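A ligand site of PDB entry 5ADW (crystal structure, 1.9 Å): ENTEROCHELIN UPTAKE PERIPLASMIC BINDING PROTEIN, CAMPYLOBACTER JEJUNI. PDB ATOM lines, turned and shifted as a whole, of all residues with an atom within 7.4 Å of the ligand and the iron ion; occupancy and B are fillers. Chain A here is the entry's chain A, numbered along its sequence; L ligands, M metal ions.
NH2 of Arg 226 is in salt-bridge range of O2 of the ligand (2.6 Å). The guanidinium group (NH2) of Arg 95 sits close to an oxygen (O4) of the ligand, at 2.8 Å. NH2 of Arg 182 sits close to O11 of the ligand. The side-chain amino group of Lys 98 sits at hydrogen-bond distance from an oxygen (O7) of the ligand, 3.3 Å away. The side-chain amide nitrogen of Gln 75 lies close to an oxygen (O10) of the ligand (3.5 Å).
The guanidinium group (NE) of Arg 226 sits close to the side-chain hydroxyl (OH) of Tyr 265 (2.7 Å). The backbone carbonyl oxygen of Tyr 265 is in hydrogen-bond range of the guanidinium group of Arg 95 (2.8 Å). The backbone carbonyl oxygen (O) of Tyr 265 sits at hydrogen-bond distance from the guanidinium group (NH2) of Arg 182, 3.2 Å away. OD1 of Asn 170 is in hydrogen-bond range of NH1 of Arg 226 (3.0 Å). The backbone carbonyl oxygen of Arg 95 sits at hydrogen-bond distance from the side-chain amino group of Lys 98, at 3.2 Å. The guanidinium group of Arg 95 sits at hydrogen-bond distance from the backbone carbonyl oxygen of Leu 266 (3.1 Å). NH1 of Arg 182 sits at hydrogen-bond distance from O of Thr 203 (3.0 Å). The side-chain amide oxygen of Gln 75 is in hydrogen-bond range of the side-chain amino group of Lys 98, 2.7 Å away.
Merely in contact with the ligand: Thr 203. Hydrophobic or aromatic side chains that line the ligand: His 204 and Tyr 265. Within 4 Å of the ligand: Gln 75, Arg 95, Lys 98, Arg 182, Thr 203, His 204, Arg 226 and Tyr 265.
Two residues have an atom within 4 Å of the iron ion: His 204 and Tyr 265. Along chain A the residues within 4 Å of the iron ion span positions 204 to 265. The nearest printed residue that does not touch the iron ion is Arg 182 (4.1 Å).
The iron ion is bound by O3 of the ligand (1.9 Å), OH of Tyr 265 (2.0 Å), O10 of the ligand (2.0 Å), O4 of the ligand (2.0 Å), O11 of the ligand (2.1 Å) and NE2 of His 204 (2.5 Å).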
ATOM      1  N   ASN A  57     -13.723  21.528  -5.562  1.00  0.00           N
ATOM      2  CA  ASN A  57     -12.368  20.923  -5.368  1.00  0.00           C
ATOM      3  C   ASN A  57     -12.157  20.533  -3.905  1.00  0.00           C
ATOM      4  O   ASN A  57     -11.124  20.831  -3.340  1.00  0.00           O
ATOM      5  CB  ASN A  57     -11.294  21.945  -5.810  1.00  0.00           C
ATOM      6  CG  ASN A  57     -11.374  22.330  -7.277  1.00  0.00           C
ATOM      7  OD1 ASN A  57     -11.714  23.477  -7.622  1.00  0.00           O
ATOM      8  ND2 ASN A  57     -11.058  21.389  -8.152  1.00  0.00           N
ATOM      9  N   VAL A  74     -11.466  26.322  -6.943  1.00  0.00           N
ATOM     10  CA  VAL A  74     -10.289  27.149  -6.679  1.00  0.00           C
ATOM     11  C   VAL A  74      -9.864  28.031  -7.888  1.00  0.00           C
ATOM     12  O   VAL A  74      -9.349  29.138  -7.722  1.00  0.00           O
ATOM     13  CB  VAL A  74      -9.138  26.268  -6.071  1.00  0.00           C
ATOM     14  CG1 VAL A  74      -8.065  27.121  -5.428  1.00  0.00           C
ATOM     15  CG2 VAL A  74      -9.673  25.326  -4.994  1.00  0.00           C
ATOM     16  N   GLN A  75     -10.136  27.538  -9.105  1.00  0.00           N
ATOM     17  CA  GLN A  75     -10.018  28.328 -10.339  1.00  0.00           C
ATOM     18  C   GLN A  75     -11.398  28.900 -10.772  1.00  0.00           C
ATOM     19  O   GLN A  75     -11.480  30.077 -11.196  1.00  0.00           O
ATOM     20  CB  GLN A  75      -9.434  27.477 -11.517  1.00  0.00           C
ATOM     21  CG  GLN A  75      -7.910  27.232 -11.649  1.00  0.00           C
ATOM     22  CD  GLN A  75      -6.954  28.424 -11.500  1.00  0.00           C
ATOM     23  OE1 GLN A  75      -7.320  29.617 -11.481  1.00  0.00           O
ATOM     24  NE2 GLN A  75      -5.678  28.070 -11.388  1.00  0.00           N
ATOM     25  N   GLN A  76     -12.451  28.076 -10.749  1.00  0.00           N
ATOM     26  CA  GLN A  76     -13.794  28.537 -11.180  1.00  0.00           C
ATOM     27  C   GLN A  76     -14.573  29.159 -10.012  1.00  0.00           C
ATOM     28  O   GLN A  76     -15.532  28.577  -9.464  1.00  0.00           O
ATOM     29  CB  GLN A  76     -14.587  27.388 -11.826  1.00  0.00           C
ATOM     30  N   SER A  93      -5.479  32.465  -1.853  1.00  0.00           N
ATOM     31  CA  SER A  93      -4.051  32.150  -2.109  1.00  0.00           C
ATOM     32  C   SER A  93      -3.777  32.458  -3.573  1.00  0.00           C
ATOM     33  O   SER A  93      -4.616  33.049  -4.250  1.00  0.00           O
ATOM     34  CB  SER A  93      -3.670  30.731  -1.711  1.00  0.00           C
ATOM     35  OG  SER A  93      -4.044  29.763  -2.648  1.00  0.00           O
ATOM     36  N   GLY A  94      -2.606  32.095  -4.074  1.00  0.00           N
ATOM     37  CA  GLY A  94      -2.195  32.568  -5.419  1.00  0.00           C
ATOM     38  C   GLY A  94      -3.115  32.256  -6.619  1.00  0.00           C
ATOM     39  O   GLY A  94      -3.147  33.014  -7.563  1.00  0.00           O
ATOM     40  N   ARG A  95      -3.854  31.145  -6.578  1.00  0.00           N
ATOM     41  CA  ARG A  95      -4.819  30.833  -7.626  1.00  0.00           C
ATOM     42  C   ARG A  95      -5.884  31.916  -7.831  1.00  0.00           C
ATOM     43  O   ARG A  95      -6.401  32.056  -8.943  1.00  0.00           O
ATOM     44  CB  ARG A  95      -5.499  29.506  -7.361  1.00  0.00           C
ATOM     45  CG  ARG A  95      -4.755  28.276  -7.864  1.00  0.00           C
ATOM     46  CD  ARG A  95      -5.662  27.034  -7.742  1.00  0.00           C
ATOM     47  NE  ARG A  95      -4.973  25.783  -8.071  1.00  0.00           N
ATOM     48  CZ  ARG A  95      -4.312  24.966  -7.234  1.00  0.00           C
ATOM     49  NH1 ARG A  95      -4.226  25.236  -5.938  1.00  0.00           N
ATOM     50  NH2 ARG A  95      -3.699  23.878  -7.738  1.00  0.00           N
ATOM     51  N   GLN A  96      -6.180  32.714  -6.809  1.00  0.00           N
ATOM     52  CA  GLN A  96      -7.254  33.726  -6.906  1.00  0.00           C
ATOM     53  C   GLN A  96      -6.754  35.152  -6.953  1.00  0.00           C
ATOM     54  O   GLN A  96      -7.550  36.102  -7.044  1.00  0.00           O
ATOM     55  CB  GLN A  96      -8.253  33.569  -5.749  1.00  0.00           C
ATOM     56  CG  GLN A  96      -8.856  32.166  -5.696  1.00  0.00           C
ATOM     57  CD  GLN A  96      -8.146  31.158  -4.800  1.00  0.00           C
ATOM     58  OE1 GLN A  96      -7.429  31.515  -3.851  1.00  0.00           O
ATOM     59  NE2 GLN A  96      -8.322  29.913  -5.100  1.00  0.00           N
ATOM     60  N   SER A  97      -5.431  35.307  -6.948  1.00  0.00           N
ATOM     61  CA  SER A  97      -4.888  36.652  -6.924  1.00  0.00           C
ATOM     62  C   SER A  97      -5.393  37.501  -8.158  1.00  0.00           C
ATOM     63  O   SER A  97      -5.598  38.715  -8.041  1.00  0.00           O
ATOM     64  CB  SER A  97      -3.393  36.554  -6.866  1.00  0.00           C
ATOM     65  OG  SER A  97      -2.940  36.955  -8.112  1.00  0.00           O
ATOM     66  N   LYS A  98      -5.610  36.854  -9.280  1.00  0.00           N
ATOM     67  CA  LYS A  98      -6.154  37.523 -10.479  1.00  0.00           C
ATOM     68  C   LYS A  98      -7.583  38.007 -10.327  1.00  0.00           C
ATOM     69  O   LYS A  98      -8.050  38.865 -11.110  1.00  0.00           O
ATOM     70  CB  LYS A  98      -6.038  36.616 -11.695  1.00  0.00           C
ATOM     71  CG  LYS A  98      -6.743  35.273 -11.564  1.00  0.00           C
ATOM     72  CD  LYS A  98      -6.639  34.485 -12.859  1.00  0.00           C
ATOM     73  CE  LYS A  98      -7.195  33.063 -12.790  1.00  0.00           C
ATOM     74  NZ  LYS A  98      -6.269  32.053 -12.165  1.00  0.00           N
ATOM     75  N   PHE A  99      -8.291  37.498  -9.293  1.00  0.00           N
ATOM     76  CA  PHE A  99      -9.638  37.969  -8.940  1.00  0.00           C
ATOM     77  C   PHE A  99      -9.679  38.920  -7.760  1.00  0.00           C
ATOM     78  O   PHE A  99     -10.761  39.247  -7.300  1.00  0.00           O
ATOM     79  CB  PHE A  99     -10.503  36.768  -8.573  1.00  0.00           C
ATOM     80  CG  PHE A  99     -10.548  35.695  -9.623  1.00  0.00           C
ATOM     81  CD1 PHE A  99     -10.787  36.020 -10.962  1.00  0.00           C
ATOM     82  CD2 PHE A  99     -10.368  34.375  -9.297  1.00  0.00           C
ATOM     83  CE1 PHE A  99     -10.784  35.026 -11.957  1.00  0.00           C
ATOM     84  CE2 PHE A  99     -10.407  33.381 -10.271  1.00  0.00           C
ATOM     85  CZ  PHE A  99     -10.618  33.699 -11.612  1.00  0.00           C
ATOM     86  N   LEU A 168       5.681  16.322 -12.478  1.00  0.00           N
ATOM     87  CA  LEU A 168       4.263  16.510 -12.602  1.00  0.00           C
ATOM     88  C   LEU A 168       3.875  15.876 -13.932  1.00  0.00           C
ATOM     89  O   LEU A 168       4.551  16.090 -14.935  1.00  0.00           O
ATOM     90  CB  LEU A 168       3.924  17.976 -12.607  1.00  0.00           C
ATOM     91  CG  LEU A 168       2.427  18.224 -12.806  1.00  0.00           C
ATOM     92  CD1 LEU A 168       1.834  18.636 -11.485  1.00  0.00           C
ATOM     93  CD2 LEU A 168       2.172  19.259 -13.875  1.00  0.00           C
ATOM     94  N   ASN A 170       0.811  15.471 -16.743  1.00  0.00           N
ATOM     95  CA  ASN A 170      -0.418  16.059 -17.261  1.00  0.00           C
ATOM     96  C   ASN A 170      -0.662  15.561 -18.706  1.00  0.00           C
ATOM     97  O   ASN A 170       0.219  15.648 -19.584  1.00  0.00           O
ATOM     98  CB  ASN A 170      -0.325  17.560 -17.232  1.00  0.00           C
ATOM     99  CG  ASN A 170      -1.546  18.208 -17.842  1.00  0.00           C
ATOM    100  OD1 ASN A 170      -2.684  17.937 -17.429  1.00  0.00           O
ATOM    101  ND2 ASN A 170      -1.335  19.048 -18.856  1.00  0.00           N
ATOM    102  N   ARG A 182       6.916  25.037  -6.431  1.00  0.00           N
ATOM    103  CA  ARG A 182       5.691  24.727  -5.668  1.00  0.00           C
ATOM    104  C   ARG A 182       5.757  23.420  -4.888  1.00  0.00           C
ATOM    105  O   ARG A 182       4.977  23.220  -3.933  1.00  0.00           O
ATOM    106  CB  ARG A 182       4.520  24.712  -6.635  1.00  0.00           C
ATOM    107  CG  ARG A 182       4.567  23.576  -7.611  1.00  0.00           C
ATOM    108  CD  ARG A 182       3.461  23.669  -8.597  1.00  0.00           C
ATOM    109  NE  ARG A 182       2.156  23.693  -7.922  1.00  0.00           N
ATOM    110  CZ  ARG A 182       1.006  23.854  -8.556  1.00  0.00           C
ATOM    111  NH1 ARG A 182       0.989  24.037  -9.862  1.00  0.00           N
ATOM    112  NH2 ARG A 182      -0.138  23.847  -7.876  1.00  0.00           N
ATOM    113  N   THR A 203       5.181  27.542 -12.825  1.00  0.00           N
ATOM    114  CA  THR A 203       3.986  27.076 -12.149  1.00  0.00           C
ATOM    115  C   THR A 203       3.669  25.611 -12.460  1.00  0.00           C
ATOM    116  O   THR A 203       3.276  24.879 -11.580  1.00  0.00           O
ATOM    117  CB  THR A 203       2.762  27.961 -12.532  1.00  0.00           C
ATOM    118  OG1 THR A 203       2.934  29.221 -11.924  1.00  0.00           O
ATOM    119  CG2 THR A 203       1.397  27.347 -12.062  1.00  0.00           C
ATOM    120  N   HIS A 204       3.773  25.248 -13.728  1.00  0.00           N
ATOM    121  CA  HIS A 204       3.522  23.885 -14.183  1.00  0.00           C
ATOM    122  C   HIS A 204       4.838  23.235 -14.740  1.00  0.00           C
ATOM    123  O   HIS A 204       4.789  22.169 -15.379  1.00  0.00           O
ATOM    124  CB  HIS A 204       2.338  23.842 -15.205  1.00  0.00           C
ATOM    125  CG  HIS A 204       1.025  24.301 -14.617  1.00  0.00           C
ATOM    126  ND1 HIS A 204       0.397  25.482 -14.999  1.00  0.00           N
ATOM    127  CD2 HIS A 204       0.225  23.753 -13.663  1.00  0.00           C
ATOM    128  CE1 HIS A 204      -0.723  25.637 -14.295  1.00  0.00           C
ATOM    129  NE2 HIS A 204      -0.844  24.603 -13.483  1.00  0.00           N
ATOM    130  N   ARG A 226      -1.334  15.282 -12.099  1.00  0.00           N
ATOM    131  CA  ARG A 226      -2.382  16.314 -12.289  1.00  0.00           C
ATOM    132  C   ARG A 226      -3.618  15.694 -12.985  1.00  0.00           C
ATOM    133  O   ARG A 226      -4.732  16.179 -12.783  1.00  0.00           O
ATOM    134  CB  ARG A 226      -1.829  17.477 -13.113  1.00  0.00           C
ATOM    135  CG  ARG A 226      -2.676  18.750 -13.261  1.00  0.00           C
ATOM    136  CD  ARG A 226      -1.840  19.768 -14.024  1.00  0.00           C
ATOM    137  NE  ARG A 226      -2.415  21.099 -14.197  1.00  0.00           N
ATOM    138  CZ  ARG A 226      -3.112  21.485 -15.270  1.00  0.00           C
ATOM    139  NH1 ARG A 226      -3.365  20.632 -16.265  1.00  0.00           N
ATOM    140  NH2 ARG A 226      -3.593  22.718 -15.331  1.00  0.00           N
ATOM    141  N   ILE A 229      -6.661  15.140 -10.769  1.00  0.00           N
ATOM    142  CA  ILE A 229      -7.453  16.313 -10.379  1.00  0.00           C
ATOM    143  C   ILE A 229      -8.350  16.750 -11.532  1.00  0.00           C
ATOM    144  O   ILE A 229      -9.472  17.143 -11.294  1.00  0.00           O
ATOM    145  CB  ILE A 229      -6.558  17.504  -9.937  1.00  0.00           C
ATOM    146  CG1 ILE A 229      -5.661  17.135  -8.741  1.00  0.00           C
ATOM    147  CG2 ILE A 229      -7.396  18.747  -9.601  1.00  0.00           C
ATOM    148  CD1 ILE A 229      -6.395  16.508  -7.558  1.00  0.00           C
ATOM    149  N   LEU A 230      -7.846  16.713 -12.771  1.00  0.00           N
ATOM    150  CA  LEU A 230      -8.601  17.140 -13.954  1.00  0.00           C
ATOM    151  C   LEU A 230      -9.517  16.057 -14.531  1.00  0.00           C
ATOM    152  O   LEU A 230     -10.265  16.313 -15.466  1.00  0.00           O
ATOM    153  CB  LEU A 230      -7.669  17.610 -15.080  1.00  0.00           C
ATOM    154  CG  LEU A 230      -6.563  18.630 -14.791  1.00  0.00           C
ATOM    155  CD1 LEU A 230      -6.050  19.259 -16.063  1.00  0.00           C
ATOM    156  CD2 LEU A 230      -7.026  19.733 -13.835  1.00  0.00           C
ATOM    157  N   TYR A 265      -0.973  18.971  -5.248  1.00  0.00           N
ATOM    158  CA  TYR A 265      -1.372  19.796  -6.370  1.00  0.00           C
ATOM    159  C   TYR A 265      -2.382  20.856  -5.940  1.00  0.00           C
ATOM    160  O   TYR A 265      -2.213  22.062  -6.205  1.00  0.00           O
ATOM    161  CB  TYR A 265      -1.959  18.971  -7.554  1.00  0.00           C
ATOM    162  CG  TYR A 265      -2.072  19.877  -8.767  1.00  0.00           C
ATOM    163  CD1 TYR A 265      -0.925  20.253  -9.458  1.00  0.00           C
ATOM    164  CD2 TYR A 265      -3.265  20.462  -9.129  1.00  0.00           C
ATOM    165  CE1 TYR A 265      -0.982  21.132 -10.541  1.00  0.00           C
ATOM    166  CE2 TYR A 265      -3.343  21.322 -10.226  1.00  0.00           C
ATOM    167  CZ  TYR A 265      -2.190  21.642 -10.928  1.00  0.00           C
ATOM    168  OH  TYR A 265      -2.233  22.555 -11.964  1.00  0.00           O
ATOM    169  N   LEU A 266      -3.423  20.434  -5.235  1.00  0.00           N
ATOM    170  CA  LEU A 266      -4.369  21.405  -4.655  1.00  0.00           C
ATOM    171  C   LEU A 266      -3.714  22.303  -3.585  1.00  0.00           C
ATOM    172  O   LEU A 266      -4.137  23.412  -3.375  1.00  0.00           O
ATOM    173  CB  LEU A 266      -5.566  20.715  -4.053  1.00  0.00           C
ATOM    174  CG  LEU A 266      -6.479  19.962  -5.001  1.00  0.00           C
ATOM    175  CD1 LEU A 266      -7.665  19.433  -4.210  1.00  0.00           C
ATOM    176  CD2 LEU A 266      -6.945  20.827  -6.174  1.00  0.00           C
ATOM    177  N   ALA A 267      -2.622  21.833  -2.989  1.00  0.00           N
ATOM    178  CA  ALA A 267      -1.618  22.683  -2.282  1.00  0.00           C
ATOM    179  C   ALA A 267      -2.146  23.167  -0.944  1.00  0.00           C
ATOM    180  O   ALA A 267      -2.297  24.372  -0.709  1.00  0.00           O
ATOM    181  CB  ALA A 267      -1.163  23.858  -3.166  1.00  0.00           C
HETATM  182  O1  LIG L   1      -4.109  25.829 -18.322  1.00  0.00           O
HETATM  183  C1  LIG L   1      -4.221  25.659 -17.089  1.00  0.00           C
HETATM  184  O2  LIG L   1      -3.310  25.091 -16.417  1.00  0.00           O
HETATM  185  C2  LIG L   1      -5.498  26.177 -16.449  1.00  0.00           C
HETATM  186  N1  LIG L   1      -5.811  25.694 -15.113  1.00  0.00           N
HETATM  187  C3  LIG L   1      -6.178  24.442 -14.787  1.00  0.00           C
HETATM  188  C4  LIG L   1      -6.330  24.155 -13.335  1.00  0.00           C
HETATM  189  C5  LIG L   1      -5.228  24.409 -12.530  1.00  0.00           C
HETATM  190  O3  LIG L   1      -4.035  24.883 -13.022  1.00  0.00           O
HETATM  191  C6  LIG L   1      -5.335  24.164 -11.190  1.00  0.00           C
HETATM  192  O4  LIG L   1      -4.231  24.450 -10.460  1.00  0.00           O
HETATM  193  C7  LIG L   1      -6.522  23.681 -10.609  1.00  0.00           C
HETATM  194  C8  LIG L   1      -7.628  23.440 -11.418  1.00  0.00           C
HETATM  195  C9  LIG L   1      -7.532  23.680 -12.786  1.00  0.00           C
HETATM  196  O5  LIG L   1      -6.330  23.540 -15.591  1.00  0.00           O
HETATM  197  C10 LIG L   1      -5.391  27.691 -16.314  1.00  0.00           C
HETATM  198  O6  LIG L   1      -4.631  27.932 -15.126  1.00  0.00           O
HETATM  199  C11 LIG L   1      -4.245  29.272 -14.664  1.00  0.00           C
HETATM  200  O7  LIG L   1      -5.047  30.190 -14.573  1.00  0.00           O
HETATM  201  C12 LIG L   1      -2.831  29.531 -14.308  1.00  0.00           C
HETATM  202  C13 LIG L   1      -1.975  29.062 -15.490  1.00  0.00           C
HETATM  203  O8  LIG L   1      -2.438  29.703 -16.689  1.00  0.00           O
HETATM  204  N2  LIG L   1      -2.560  28.817 -13.064  1.00  0.00           N
HETATM  205  C14 LIG L   1      -2.388  29.448 -11.897  1.00  0.00           C
HETATM  206  O9  LIG L   1      -2.429  30.647 -11.801  1.00  0.00           O
HETATM  207  C15 LIG L   1      -1.976  28.627 -10.724  1.00  0.00           C
HETATM  208  C16 LIG L   1      -2.083  27.235 -10.815  1.00  0.00           C
HETATM  209  O10 LIG L   1      -2.608  26.517 -11.888  1.00  0.00           O
HETATM  210  C17 LIG L   1      -1.424  29.281  -9.582  1.00  0.00           C
HETATM  211  C18 LIG L   1      -0.991  28.517  -8.502  1.00  0.00           C
HETATM  212  C19 LIG L   1      -1.090  27.123  -8.582  1.00  0.00           C
HETATM  213  C20 LIG L   1      -1.640  26.509  -9.744  1.00  0.00           C
HETATM  214  O11 LIG L   1      -1.733  25.158  -9.891  1.00  0.00           O
HETATM  215 FE    FE M   1      -2.639  24.498 -11.723  1.00  0.00          FE
